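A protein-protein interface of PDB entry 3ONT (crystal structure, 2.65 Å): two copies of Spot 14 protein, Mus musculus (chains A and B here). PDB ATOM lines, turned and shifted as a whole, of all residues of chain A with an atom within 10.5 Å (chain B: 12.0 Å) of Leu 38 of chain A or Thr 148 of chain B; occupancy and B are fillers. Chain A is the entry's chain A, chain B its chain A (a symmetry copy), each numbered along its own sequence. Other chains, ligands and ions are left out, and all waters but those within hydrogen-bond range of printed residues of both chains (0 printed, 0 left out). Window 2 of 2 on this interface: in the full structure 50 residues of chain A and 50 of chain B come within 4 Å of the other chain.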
ATOM      1  N   GLN A  31     -12.665  -6.961 -13.656  1.00  0.00           N
ATOM      2  CA  GLN A  31     -12.687  -5.830 -12.729  1.00  0.00           C
ATOM      3  C   GLN A  31     -11.843  -4.715 -13.301  1.00  0.00           C
ATOM      4  O   GLN A  31     -12.238  -3.564 -13.242  1.00  0.00           O
ATOM      5  CB  GLN A  31     -12.149  -6.173 -11.342  1.00  0.00           C
ATOM      6  CG  GLN A  31     -12.769  -7.387 -10.669  1.00  0.00           C
ATOM      7  CD  GLN A  31     -14.244  -7.211 -10.329  1.00  0.00           C
ATOM      8  OE1 GLN A  31     -14.694  -6.117  -9.938  1.00  0.00           O
ATOM      9  NE2 GLN A  31     -15.006  -8.304 -10.445  1.00  0.00           N
ATOM     10  N   VAL A  32     -10.687  -5.066 -13.856  1.00  0.00           N
ATOM     11  CA  VAL A  32      -9.700  -4.092 -14.340  1.00  0.00           C
ATOM     12  C   VAL A  32     -10.131  -3.373 -15.622  1.00  0.00           C
ATOM     13  O   VAL A  32      -9.989  -2.142 -15.741  1.00  0.00           O
ATOM     14  CB  VAL A  32      -8.315  -4.760 -14.547  1.00  0.00           C
ATOM     15  CG1 VAL A  32      -7.381  -3.880 -15.365  1.00  0.00           C
ATOM     16  CG2 VAL A  32      -7.688  -5.120 -13.200  1.00  0.00           C
ATOM     17  N   VAL A  33     -10.658  -4.134 -16.576  1.00  0.00           N
ATOM     18  CA  VAL A  33     -11.036  -3.583 -17.876  1.00  0.00           C
ATOM     19  C   VAL A  33     -12.352  -2.829 -17.743  1.00  0.00           C
ATOM     20  O   VAL A  33     -13.413  -3.303 -18.129  1.00  0.00           O
ATOM     21  CB  VAL A  33     -11.063  -4.683 -18.983  1.00  0.00           C
ATOM     22  CG1 VAL A  33     -11.547  -4.127 -20.293  1.00  0.00           C
ATOM     23  CG2 VAL A  33      -9.658  -5.291 -19.159  1.00  0.00           C
ATOM     24  N   MET A  34     -12.259  -1.627 -17.191  1.00  0.00           N
ATOM     25  CA  MET A  34     -13.430  -0.828 -16.845  1.00  0.00           C
ATOM     26  C   MET A  34     -14.184  -0.314 -18.066  1.00  0.00           C
ATOM     27  O   MET A  34     -15.423  -0.221 -18.040  1.00  0.00           O
ATOM     28  CB  MET A  34     -12.991   0.360 -16.002  1.00  0.00           C
ATOM     29  CG  MET A  34     -12.318  -0.026 -14.696  1.00  0.00           C
ATOM     30  SD  MET A  34     -13.490   0.263 -13.164  1.00  0.00           S
ATOM     31  CE  MET A  34     -14.838  -1.124 -13.508  1.00  0.00           C
ATOM     32  N   ILE A  35     -13.436   0.051 -19.113  1.00  0.00           N
ATOM     33  CA  ILE A  35     -14.014   0.597 -20.336  1.00  0.00           C
ATOM     34  C   ILE A  35     -13.585  -0.326 -21.488  1.00  0.00           C
ATOM     35  O   ILE A  35     -12.553  -0.103 -22.154  1.00  0.00           O
ATOM     36  CB  ILE A  35     -13.595   2.098 -20.580  1.00  0.00           C
ATOM     37  CG1 ILE A  35     -13.674   2.917 -19.279  1.00  0.00           C
ATOM     38  CG2 ILE A  35     -14.443   2.734 -21.700  1.00  0.00           C
ATOM     39  CD1 ILE A  35     -13.077   4.310 -19.353  1.00  0.00           C
ATOM     40  N   PRO A  36     -14.373  -1.384 -21.721  1.00  0.00           N
ATOM     41  CA  PRO A  36     -13.948  -2.430 -22.661  1.00  0.00           C
ATOM     42  C   PRO A  36     -13.872  -1.947 -24.108  1.00  0.00           C
ATOM     43  O   PRO A  36     -13.158  -2.547 -24.918  1.00  0.00           O
ATOM     44  CB  PRO A  36     -15.025  -3.531 -22.491  1.00  0.00           C
ATOM     45  CG  PRO A  36     -15.643  -3.268 -21.128  1.00  0.00           C
ATOM     46  CD  PRO A  36     -15.622  -1.742 -21.012  1.00  0.00           C
ATOM     47  N   SER A  37     -14.583  -0.870 -24.440  1.00  0.00           N
ATOM     48  CA  SER A  37     -14.576  -0.343 -25.825  1.00  0.00           C
ATOM     49  C   SER A  37     -13.201   0.229 -26.209  1.00  0.00           C
ATOM     50  O   SER A  37     -12.893   0.329 -27.381  1.00  0.00           O
ATOM     51  CB  SER A  37     -15.652   0.712 -26.011  1.00  0.00           C
ATOM     52  OG  SER A  37     -15.416   1.746 -25.079  1.00  0.00           O
ATOM     53  N   LEU A  38     -12.379   0.576 -25.221  1.00  0.00           N
ATOM     54  CA  LEU A  38     -10.987   0.983 -25.452  1.00  0.00           C
ATOM     55  C   LEU A  38     -10.144  -0.150 -26.084  1.00  0.00           C
ATOM     56  O   LEU A  38      -9.091   0.120 -26.688  1.00  0.00           O
ATOM     57  CB  LEU A  38     -10.328   1.469 -24.144  1.00  0.00           C
ATOM     58  CG  LEU A  38     -10.988   2.688 -23.480  1.00  0.00           C
ATOM     59  CD1 LEU A  38     -10.148   3.160 -22.310  1.00  0.00           C
ATOM     60  CD2 LEU A  38     -11.277   3.878 -24.444  1.00  0.00           C
ATOM     61  N   LEU A  39     -10.593  -1.400 -25.932  1.00  0.00           N
ATOM     62  CA  LEU A  39      -9.915  -2.552 -26.542  1.00  0.00           C
ATOM     63  C   LEU A  39     -10.226  -2.700 -28.029  1.00  0.00           C
ATOM     64  O   LEU A  39      -9.496  -3.385 -28.746  1.00  0.00           O
ATOM     65  CB  LEU A  39     -10.270  -3.853 -25.817  1.00  0.00           C
ATOM     66  CG  LEU A  39      -9.910  -4.016 -24.336  1.00  0.00           C
ATOM     67  CD1 LEU A  39     -10.416  -5.355 -23.753  1.00  0.00           C
ATOM     68  CD2 LEU A  39      -8.396  -3.904 -24.110  1.00  0.00           C
ATOM     69  N   ARG A  40     -11.293  -2.076 -28.515  1.00  0.00           N
ATOM     70  CA  ARG A  40     -11.600  -2.150 -29.958  1.00  0.00           C
ATOM     71  C   ARG A  40     -10.424  -1.543 -30.700  1.00  0.00           C
ATOM     72  O   ARG A  40      -9.802  -0.574 -30.215  1.00  0.00           O
ATOM     73  CB  ARG A  40     -12.829  -1.333 -30.308  1.00  0.00           C
ATOM     74  CG  ARG A  40     -14.084  -1.739 -29.639  1.00  0.00           C
ATOM     75  CD  ARG A  40     -14.952  -2.468 -30.588  1.00  0.00           C
ATOM     76  NE  ARG A  40     -16.274  -2.719 -30.022  1.00  0.00           N
ATOM     77  CZ  ARG A  40     -17.105  -3.663 -30.452  1.00  0.00           C
ATOM     78  NH1 ARG A  40     -16.751  -4.464 -31.445  1.00  0.00           N
ATOM     79  NH2 ARG A  40     -18.284  -3.824 -29.881  1.00  0.00           N
ATOM     80  N   ASP A  41     -10.102  -2.122 -31.850  1.00  0.00           N
ATOM     81  CA  ASP A  41      -9.062  -1.586 -32.738  1.00  0.00           C
ATOM     82  C   ASP A  41      -7.628  -1.742 -32.245  1.00  0.00           C
ATOM     83  O   ASP A  41      -6.726  -1.104 -32.790  1.00  0.00           O
ATOM     84  CB  ASP A  41      -9.323  -0.112 -33.029  1.00  0.00           C
ATOM     85  CG  ASP A  41     -10.643   0.114 -33.719  1.00  0.00           C
ATOM     86  OD1 ASP A  41     -11.070  -0.812 -34.463  1.00  0.00           O
ATOM     87  OD2 ASP A  41     -11.234   1.215 -33.521  1.00  0.00           O
ATOM     88  N   VAL A  42      -7.420  -2.531 -31.190  1.00  0.00           N
ATOM     89  CA  VAL A  42      -6.075  -2.872 -30.734  1.00  0.00           C
ATOM     90  C   VAL A  42      -5.817  -4.207 -31.377  1.00  0.00           C
ATOM     91  O   VAL A  42      -6.577  -5.161 -31.160  1.00  0.00           O
ATOM     92  CB  VAL A  42      -5.964  -2.994 -29.200  1.00  0.00           C
ATOM     93  CG1 VAL A  42      -4.601  -3.556 -28.802  1.00  0.00           C
ATOM     94  CG2 VAL A  42      -6.198  -1.648 -28.530  1.00  0.00           C
ATOM     95  N   GLN A  43      -4.766  -4.257 -32.198  1.00  0.00           N
ATOM     96  CA  GLN A  43      -4.459  -5.450 -32.981  1.00  0.00           C
ATOM     97  C   GLN A  43      -3.973  -6.629 -32.155  1.00  0.00           C
ATOM     98  O   GLN A  43      -3.290  -6.466 -31.138  1.00  0.00           O
ATOM     99  CB  GLN A  43      -3.512  -5.138 -34.140  1.00  0.00           C
ATOM    100  CG  GLN A  43      -4.238  -4.572 -35.369  1.00  0.00           C
ATOM    101  CD  GLN A  43      -5.705  -5.052 -35.514  1.00  0.00           C
ATOM    102  OE1 GLN A  43      -6.577  -4.261 -35.903  1.00  0.00           O
ATOM    103  NE2 GLN A  43      -5.978  -6.349 -35.192  1.00  0.00           N
ATOM    104  N   ASP A  57     -10.051  -8.315 -33.234  1.00  0.00           N
ATOM    105  CA  ASP A  57      -9.078  -7.547 -32.465  1.00  0.00           C
ATOM    106  C   ASP A  57      -9.056  -7.978 -30.997  1.00  0.00           C
ATOM    107  O   ASP A  57      -9.689  -8.967 -30.606  1.00  0.00           O
ATOM    108  CB  ASP A  57      -9.390  -6.051 -32.565  1.00  0.00           C
ATOM    109  CG  ASP A  57     -10.835  -5.700 -32.119  1.00  0.00           C
ATOM    110  OD1 ASP A  57     -11.332  -4.612 -32.508  1.00  0.00           O
ATOM    111  OD2 ASP A  57     -11.486  -6.486 -31.384  1.00  0.00           O
ATOM    112  N   LEU A  58      -8.359  -7.197 -30.178  1.00  0.00           N
ATOM    113  CA  LEU A  58      -8.260  -7.451 -28.749  1.00  0.00           C
ATOM    114  C   LEU A  58      -9.619  -7.515 -28.054  1.00  0.00           C
ATOM    115  O   LEU A  58      -9.802  -8.306 -27.134  1.00  0.00           O
ATOM    116  CB  LEU A  58      -7.382  -6.405 -28.087  1.00  0.00           C
ATOM    117  CG  LEU A  58      -6.820  -6.846 -26.742  1.00  0.00           C
ATOM    118  CD1 LEU A  58      -6.232  -8.272 -26.829  1.00  0.00           C
ATOM    119  CD2 LEU A  58      -5.778  -5.848 -26.241  1.00  0.00           C
ATOM    120  N   TYR A  59     -10.583  -6.702 -28.477  1.00  0.00           N
ATOM    121  CA  TYR A  59     -11.895  -6.793 -27.865  1.00  0.00           C
ATOM    122  C   TYR A  59     -12.573  -8.137 -28.147  1.00  0.00           C
ATOM    123  O   TYR A  59     -13.258  -8.689 -27.265  1.00  0.00           O
ATOM    124  CB  TYR A  59     -12.788  -5.615 -28.256  1.00  0.00           C
ATOM    125  CG  TYR A  59     -14.197  -5.750 -27.726  1.00  0.00           C
ATOM    126  CD1 TYR A  59     -14.516  -5.357 -26.427  1.00  0.00           C
ATOM    127  CD2 TYR A  59     -15.204  -6.309 -28.517  1.00  0.00           C
ATOM    128  CE1 TYR A  59     -15.801  -5.500 -25.940  1.00  0.00           C
ATOM    129  CE2 TYR A  59     -16.485  -6.463 -28.039  1.00  0.00           C
ATOM    130  CZ  TYR A  59     -16.781  -6.055 -26.757  1.00  0.00           C
ATOM    131  OH  TYR A  59     -18.066  -6.209 -26.290  1.00  0.00           O
ATOM    132  N   THR A  60     -12.388  -8.670 -29.352  1.00  0.00           N
ATOM    133  CA  THR A  60     -12.940  -9.965 -29.722  1.00  0.00           C
ATOM    134  C   THR A  60     -12.320 -11.050 -28.845  1.00  0.00           C
ATOM    135  O   THR A  60     -12.989 -11.997 -28.417  1.00  0.00           O
ATOM    136  CB  THR A  60     -12.609 -10.303 -31.180  1.00  0.00           C
ATOM    137  OG1 THR A  60     -12.833  -9.148 -31.996  1.00  0.00           O
ATOM    138  CG2 THR A  60     -13.456 -11.464 -31.694  1.00  0.00           C
ATOM    139  N   PHE A  62     -10.717 -10.650 -25.762  1.00  0.00           N
ATOM    140  CA  PHE A  62     -11.289 -10.409 -24.454  1.00  0.00           C
ATOM    141  C   PHE A  62     -12.670 -11.097 -24.345  1.00  0.00           C
ATOM    142  O   PHE A  62     -12.930 -11.858 -23.417  1.00  0.00           O
ATOM    143  CB  PHE A  62     -11.356  -8.888 -24.300  1.00  0.00           C
ATOM    144  CG  PHE A  62     -12.135  -8.401 -23.133  1.00  0.00           C
ATOM    145  CD1 PHE A  62     -11.578  -8.377 -21.870  1.00  0.00           C
ATOM    146  CD2 PHE A  62     -13.412  -7.866 -23.316  1.00  0.00           C
ATOM    147  CE1 PHE A  62     -12.301  -7.859 -20.781  1.00  0.00           C
ATOM    148  CE2 PHE A  62     -14.147  -7.356 -22.247  1.00  0.00           C
ATOM    149  CZ  PHE A  62     -13.590  -7.355 -20.977  1.00  0.00           C
ATOM    150  N   GLU B 139      -2.062 -10.927 -19.898  1.00  0.00           N
ATOM    151  CA  GLU B 139      -1.488  -9.974 -20.837  1.00  0.00           C
ATOM    152  C   GLU B 139      -2.515  -8.929 -21.270  1.00  0.00           C
ATOM    153  O   GLU B 139      -2.162  -7.762 -21.462  1.00  0.00           O
ATOM    154  CB  GLU B 139      -0.861 -10.682 -22.040  1.00  0.00           C
ATOM    155  CG  GLU B 139       0.534 -11.252 -21.738  1.00  0.00           C
ATOM    156  CD  GLU B 139       1.018 -12.291 -22.761  1.00  0.00           C
ATOM    157  OE1 GLU B 139       0.333 -12.502 -23.800  1.00  0.00           O
ATOM    158  OE2 GLU B 139       2.088 -12.904 -22.522  1.00  0.00           O
ATOM    159  N   VAL B 140      -3.781  -9.334 -21.390  1.00  0.00           N
ATOM    160  CA  VAL B 140      -4.827  -8.376 -21.695  1.00  0.00           C
ATOM    161  C   VAL B 140      -4.990  -7.370 -20.550  1.00  0.00           C
ATOM    162  O   VAL B 140      -5.154  -6.177 -20.796  1.00  0.00           O
ATOM    163  CB  VAL B 140      -6.183  -9.024 -21.975  1.00  0.00           C
ATOM    164  CG1 VAL B 140      -7.250  -7.915 -22.154  1.00  0.00           C
ATOM    165  CG2 VAL B 140      -6.115  -9.936 -23.195  1.00  0.00           C
ATOM    166  N   THR B 141      -4.946  -7.858 -19.311  1.00  0.00           N
ATOM    167  CA  THR B 141      -5.085  -7.010 -18.125  1.00  0.00           C
ATOM    168  C   THR B 141      -3.946  -6.008 -18.072  1.00  0.00           C
ATOM    169  O   THR B 141      -4.173  -4.826 -17.878  1.00  0.00           O
ATOM    170  CB  THR B 141      -5.085  -7.855 -16.830  1.00  0.00           C
ATOM    171  OG1 THR B 141      -6.143  -8.810 -16.894  1.00  0.00           O
ATOM    172  CG2 THR B 141      -5.291  -6.995 -15.619  1.00  0.00           C
ATOM    173  N   ARG B 142      -2.720  -6.496 -18.244  1.00  0.00           N
ATOM    174  CA  ARG B 142      -1.540  -5.645 -18.289  1.00  0.00           C
ATOM    175  C   ARG B 142      -1.656  -4.573 -19.401  1.00  0.00           C
ATOM    176  O   ARG B 142      -1.353  -3.397 -19.176  1.00  0.00           O
ATOM    177  CB  ARG B 142      -0.278  -6.502 -18.490  1.00  0.00           C
ATOM    178  CG  ARG B 142       1.035  -5.774 -18.185  1.00  0.00           C
ATOM    179  CD  ARG B 142       1.077  -5.390 -16.695  1.00  0.00           C
ATOM    180  NE  ARG B 142       1.836  -4.169 -16.354  1.00  0.00           N
ATOM    181  CZ  ARG B 142       2.962  -4.162 -15.625  1.00  0.00           C
ATOM    182  NH1 ARG B 142       3.487  -5.310 -15.180  1.00  0.00           N
ATOM    183  NH2 ARG B 142       3.573  -3.008 -15.341  1.00  0.00           N
ATOM    184  N   LYS B 143      -2.120  -4.984 -20.582  1.00  0.00           N
ATOM    185  CA  LYS B 143      -2.214  -4.098 -21.720  1.00  0.00           C
ATOM    186  C   LYS B 143      -3.171  -2.948 -21.417  1.00  0.00           C
ATOM    187  O   LYS B 143      -2.840  -1.784 -21.644  1.00  0.00           O
ATOM    188  CB  LYS B 143      -2.603  -4.867 -22.988  1.00  0.00           C
ATOM    189  CG  LYS B 143      -2.739  -3.997 -24.232  1.00  0.00           C
ATOM    190  CD  LYS B 143      -1.620  -4.160 -25.271  1.00  0.00           C
ATOM    191  CE  LYS B 143      -0.515  -3.093 -25.158  1.00  0.00           C
ATOM    192  NZ  LYS B 143      -0.870  -1.742 -25.677  1.00  0.00           N
ATOM    193  N   TYR B 144      -4.340  -3.270 -20.881  1.00  0.00           N
ATOM    194  CA  TYR B 144      -5.306  -2.236 -20.488  1.00  0.00           C
ATOM    195  C   TYR B 144      -4.748  -1.260 -19.455  1.00  0.00           C
ATOM    196  O   TYR B 144      -4.960  -0.050 -19.545  1.00  0.00           O
ATOM    197  CB  TYR B 144      -6.566  -2.864 -19.922  1.00  0.00           C
ATOM    198  CG  TYR B 144      -7.657  -1.859 -19.654  1.00  0.00           C
ATOM    199  CD1 TYR B 144      -7.762  -1.228 -18.415  1.00  0.00           C
ATOM    200  CD2 TYR B 144      -8.598  -1.538 -20.644  1.00  0.00           C
ATOM    201  CE1 TYR B 144      -8.771  -0.323 -18.166  1.00  0.00           C
ATOM    202  CE2 TYR B 144      -9.607  -0.633 -20.403  1.00  0.00           C
ATOM    203  CZ  TYR B 144      -9.690  -0.027 -19.163  1.00  0.00           C
ATOM    204  OH  TYR B 144     -10.704   0.876 -18.912  1.00  0.00           O
ATOM    205  N   GLN B 145      -4.058  -1.793 -18.451  1.00  0.00           N
ATOM    206  CA  GLN B 145      -3.431  -0.950 -17.442  1.00  0.00           C
ATOM    207  C   GLN B 145      -2.432  -0.018 -18.103  1.00  0.00           C
ATOM    208  O   GLN B 145      -2.412   1.175 -17.803  1.00  0.00           O
ATOM    209  CB  GLN B 145      -2.784  -1.794 -16.346  1.00  0.00           C
ATOM    210  CG  GLN B 145      -3.811  -2.423 -15.422  1.00  0.00           C
ATOM    211  CD  GLN B 145      -3.243  -3.520 -14.503  1.00  0.00           C
ATOM    212  OE1 GLN B 145      -2.164  -4.073 -14.733  1.00  0.00           O
ATOM    213  NE2 GLN B 145      -3.989  -3.832 -13.454  1.00  0.00           N
ATOM    214  N   GLU B 146      -1.649  -0.562 -19.035  1.00  0.00           N
ATOM    215  CA  GLU B 146      -0.672   0.221 -19.782  1.00  0.00           C
ATOM    216  C   GLU B 146      -1.372   1.317 -20.583  1.00  0.00           C
ATOM    217  O   GLU B 146      -1.075   2.508 -20.407  1.00  0.00           O
ATOM    218  CB  GLU B 146       0.192  -0.680 -20.674  1.00  0.00           C
ATOM    219  CG  GLU B 146       1.418  -1.283 -19.962  1.00  0.00           C
ATOM    220  CD  GLU B 146       2.095  -2.446 -20.728  1.00  0.00           C
ATOM    221  OE1 GLU B 146       1.855  -2.618 -21.949  1.00  0.00           O
ATOM    222  OE2 GLU B 146       2.887  -3.200 -20.105  1.00  0.00           O
ATOM    223  N   MET B 147      -2.335   0.911 -21.409  1.00  0.00           N
ATOM    224  CA  MET B 147      -3.117   1.828 -22.248  1.00  0.00           C
ATOM    225  C   MET B 147      -3.716   2.994 -21.503  1.00  0.00           C
ATOM    226  O   MET B 147      -3.786   4.093 -22.032  1.00  0.00           O
ATOM    227  CB  MET B 147      -4.268   1.095 -22.903  1.00  0.00           C
ATOM    228  CG  MET B 147      -3.869   0.226 -24.041  1.00  0.00           C
ATOM    229  SD  MET B 147      -5.356  -0.938 -24.447  1.00  0.00           S
ATOM    230  CE  MET B 147      -6.792   0.343 -24.292  1.00  0.00           C
ATOM    231  N   THR B 148      -4.193   2.755 -20.293  1.00  0.00           N
ATOM    232  CA  THR B 148      -4.864   3.819 -19.574  1.00  0.00           C
ATOM    233  C   THR B 148      -3.927   4.392 -18.519  1.00  0.00           C
ATOM    234  O   THR B 148      -4.375   4.917 -17.497  1.00  0.00           O
ATOM    235  CB  THR B 148      -6.166   3.337 -18.942  1.00  0.00           C
ATOM    236  OG1 THR B 148      -5.876   2.300 -18.000  1.00  0.00           O
ATOM    237  CG2 THR B 148      -7.104   2.799 -20.000  1.00  0.00           C
ATOM    238  N   GLY B 149      -2.622   4.257 -18.771  1.00  0.00           N
ATOM    239  CA  GLY B 149      -1.569   4.822 -17.925  1.00  0.00           C
ATOM    240  C   GLY B 149      -1.610   4.524 -16.433  1.00  0.00           C
ATOM    241  O   GLY B 149      -1.213   5.371 -15.640  1.00  0.00           O
ATOM    242  N   GLN B 150      -2.091   3.340 -16.041  1.00  0.00           N
ATOM    243  CA  GLN B 150      -2.011   2.899 -14.635  1.00  0.00           C
ATOM    244  C   GLN B 150      -0.596   2.448 -14.236  1.00  0.00           C
ATOM    245  O   GLN B 150      -0.249   2.458 -13.051  1.00  0.00           O
ATOM    246  CB  GLN B 150      -3.022   1.784 -14.329  1.00  0.00           C
ATOM    247  CG  GLN B 150      -4.454   2.261 -14.116  1.00  0.00           C
ATOM    248  CD  GLN B 150      -5.477   1.142 -14.259  1.00  0.00           C
ATOM    249  OE1 GLN B 150      -5.406   0.114 -13.575  1.00  0.00           O
ATOM    250  NE2 GLN B 150      -6.440   1.340 -15.154  1.00  0.00           N
ATOM    251  N   VAL B 151       0.202   2.027 -15.222  1.00  0.00           N
ATOM    252  CA  VAL B 151       1.628   1.742 -15.006  1.00  0.00           C
ATOM    253  C   VAL B 151       2.471   2.441 -16.074  1.00  0.00           C
ATOM    254  O   VAL B 151       2.746   1.872 -17.133  1.00  0.00           O
ATOM    255  CB  VAL B 151       1.975   0.219 -15.003  1.00  0.00           C
ATOM    256  CG1 VAL B 151       3.232  -0.034 -14.140  1.00  0.00           C
ATOM    257  CG2 VAL B 151       0.798  -0.641 -14.520  1.00  0.00           C
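The side-chain hydroxyl (OH) of Tyr 144 of chain B lies within hydrogen-bond range of the backbone NH (N) of Met 34 of chain A (3.4 Å).
OH of Tyr 144 of chain B lies within hydrogen-bond range of N of Ile 35 of chain A, at 2.9 Å.
O of Val 42 of chain A sits at hydrogen-bond distance from N of Leu 58 of chain A (2.9 Å).
O of Tyr 144 of chain B is in hydrogen-bond range of OG1 of Thr 148 of chain B (3.0 Å).
The backbone NH (N) of Gln 150 of chain B is in hydrogen-bond range of the backbone carbonyl oxygen (O) of Gln 145 of chain B, at 2.8 Å.
OG1 of Thr 148 of chain B sits at hydrogen-bond distance from NE2 of Gln 150 of chain B.
CG2 of Thr 141 of chain B touches CG1 of Val 32 of chain A, at 3.8 Å.
Val 32 of chain A touches Tyr 144 of chain B (O to CE1, 3.3 Å).
Gln 145 of chain B touches Val 32 of chain A.
CG1 of Val 33 of chain A touches CD2 of Tyr 144 of chain B, at 3.9 Å.
Met 147 of chain B touches Leu 38 of chain A (CE to O, 3.3 Å).
Thr 148 of chain B touches Leu 38 of chain A (CG2 to CD1, 3.8 Å).
CD1 of Leu 58 of chain A touches CG2 of Val 140 of chain B, at 3.999 Å.
Of chain B, only Met 147 (3.3 Å) and Thr 148 (3.8 Å) come within 4 Å of Leu 38 of chain A.
Thr 148 of chain B touches just one residue of chain A: Leu 38 (3.8 Å).
Of chain B, only Tyr 144 (2.9 Å) comes within 4 Å of Ile 35 of chain A.
Pro 36 of chain A touches none of the printed residues of chain B.
No residue of chain B comes within 4 Å of Ser 37 of chain A.
No residue of chain B comes within 4 Å of Val 42 of chain A.
Of chain A, only Leu 38 comes within 4 Å of Met 147 of chain B.
No residue of chain A comes within 4 Å of Gly 149 of chain B.
Printed residues of chain A within 4 Å of Gln 145 of chain B: Val 32.
Of the printed residues of chain A, Val 140 of chain B touches Leu 58.
Of the printed residues of chain B, Met 34 of chain A touches Tyr 144.
Of the printed residues of chain B, Val 32 of chain A touches Thr 141, Tyr 144 and Gln 145.
Printed residues of chain B within 4 Å of Leu 58 of chain A: Val 140.
The nearest residue of chain B that does not touch Leu 38 of chain A is Tyr 144 of chain B (4.1 Å).
The nearest residue of chain A that does not touch Thr 148 of chain B is Ile 35 of chain A (6.2 Å).
Hydrophobic or aromatic side chains of chain B that line the printed part of chain A: Val 140, Tyr 144 and Met 147.
Along chain B the printed residues that touch a printed residue of chain A span positions 140 to 148.
Of the 18 printed residues of chain A, 6 touch a printed residue of chain B.
Printed residues of chain A that touch a printed residue of chain B: Val 32, Val 33, Met 34, Ile 35, Leu 38 and Leu 58.
Hydrophobic or aromatic side chains of chain A that line the printed part of chain B: Val 32, Val 33, Met 34, Ile 35, Leu 38 and Leu 58.
Among the printed residues, no Asp or Glu carboxylate lies within 4 Å of a Lys or Arg side-chain nitrogen of the other chain.
No position is printed for both chains.
Of the 9 pairs that touch across the chains among the printed residues, none has its exchanged pair printed and touching as well.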
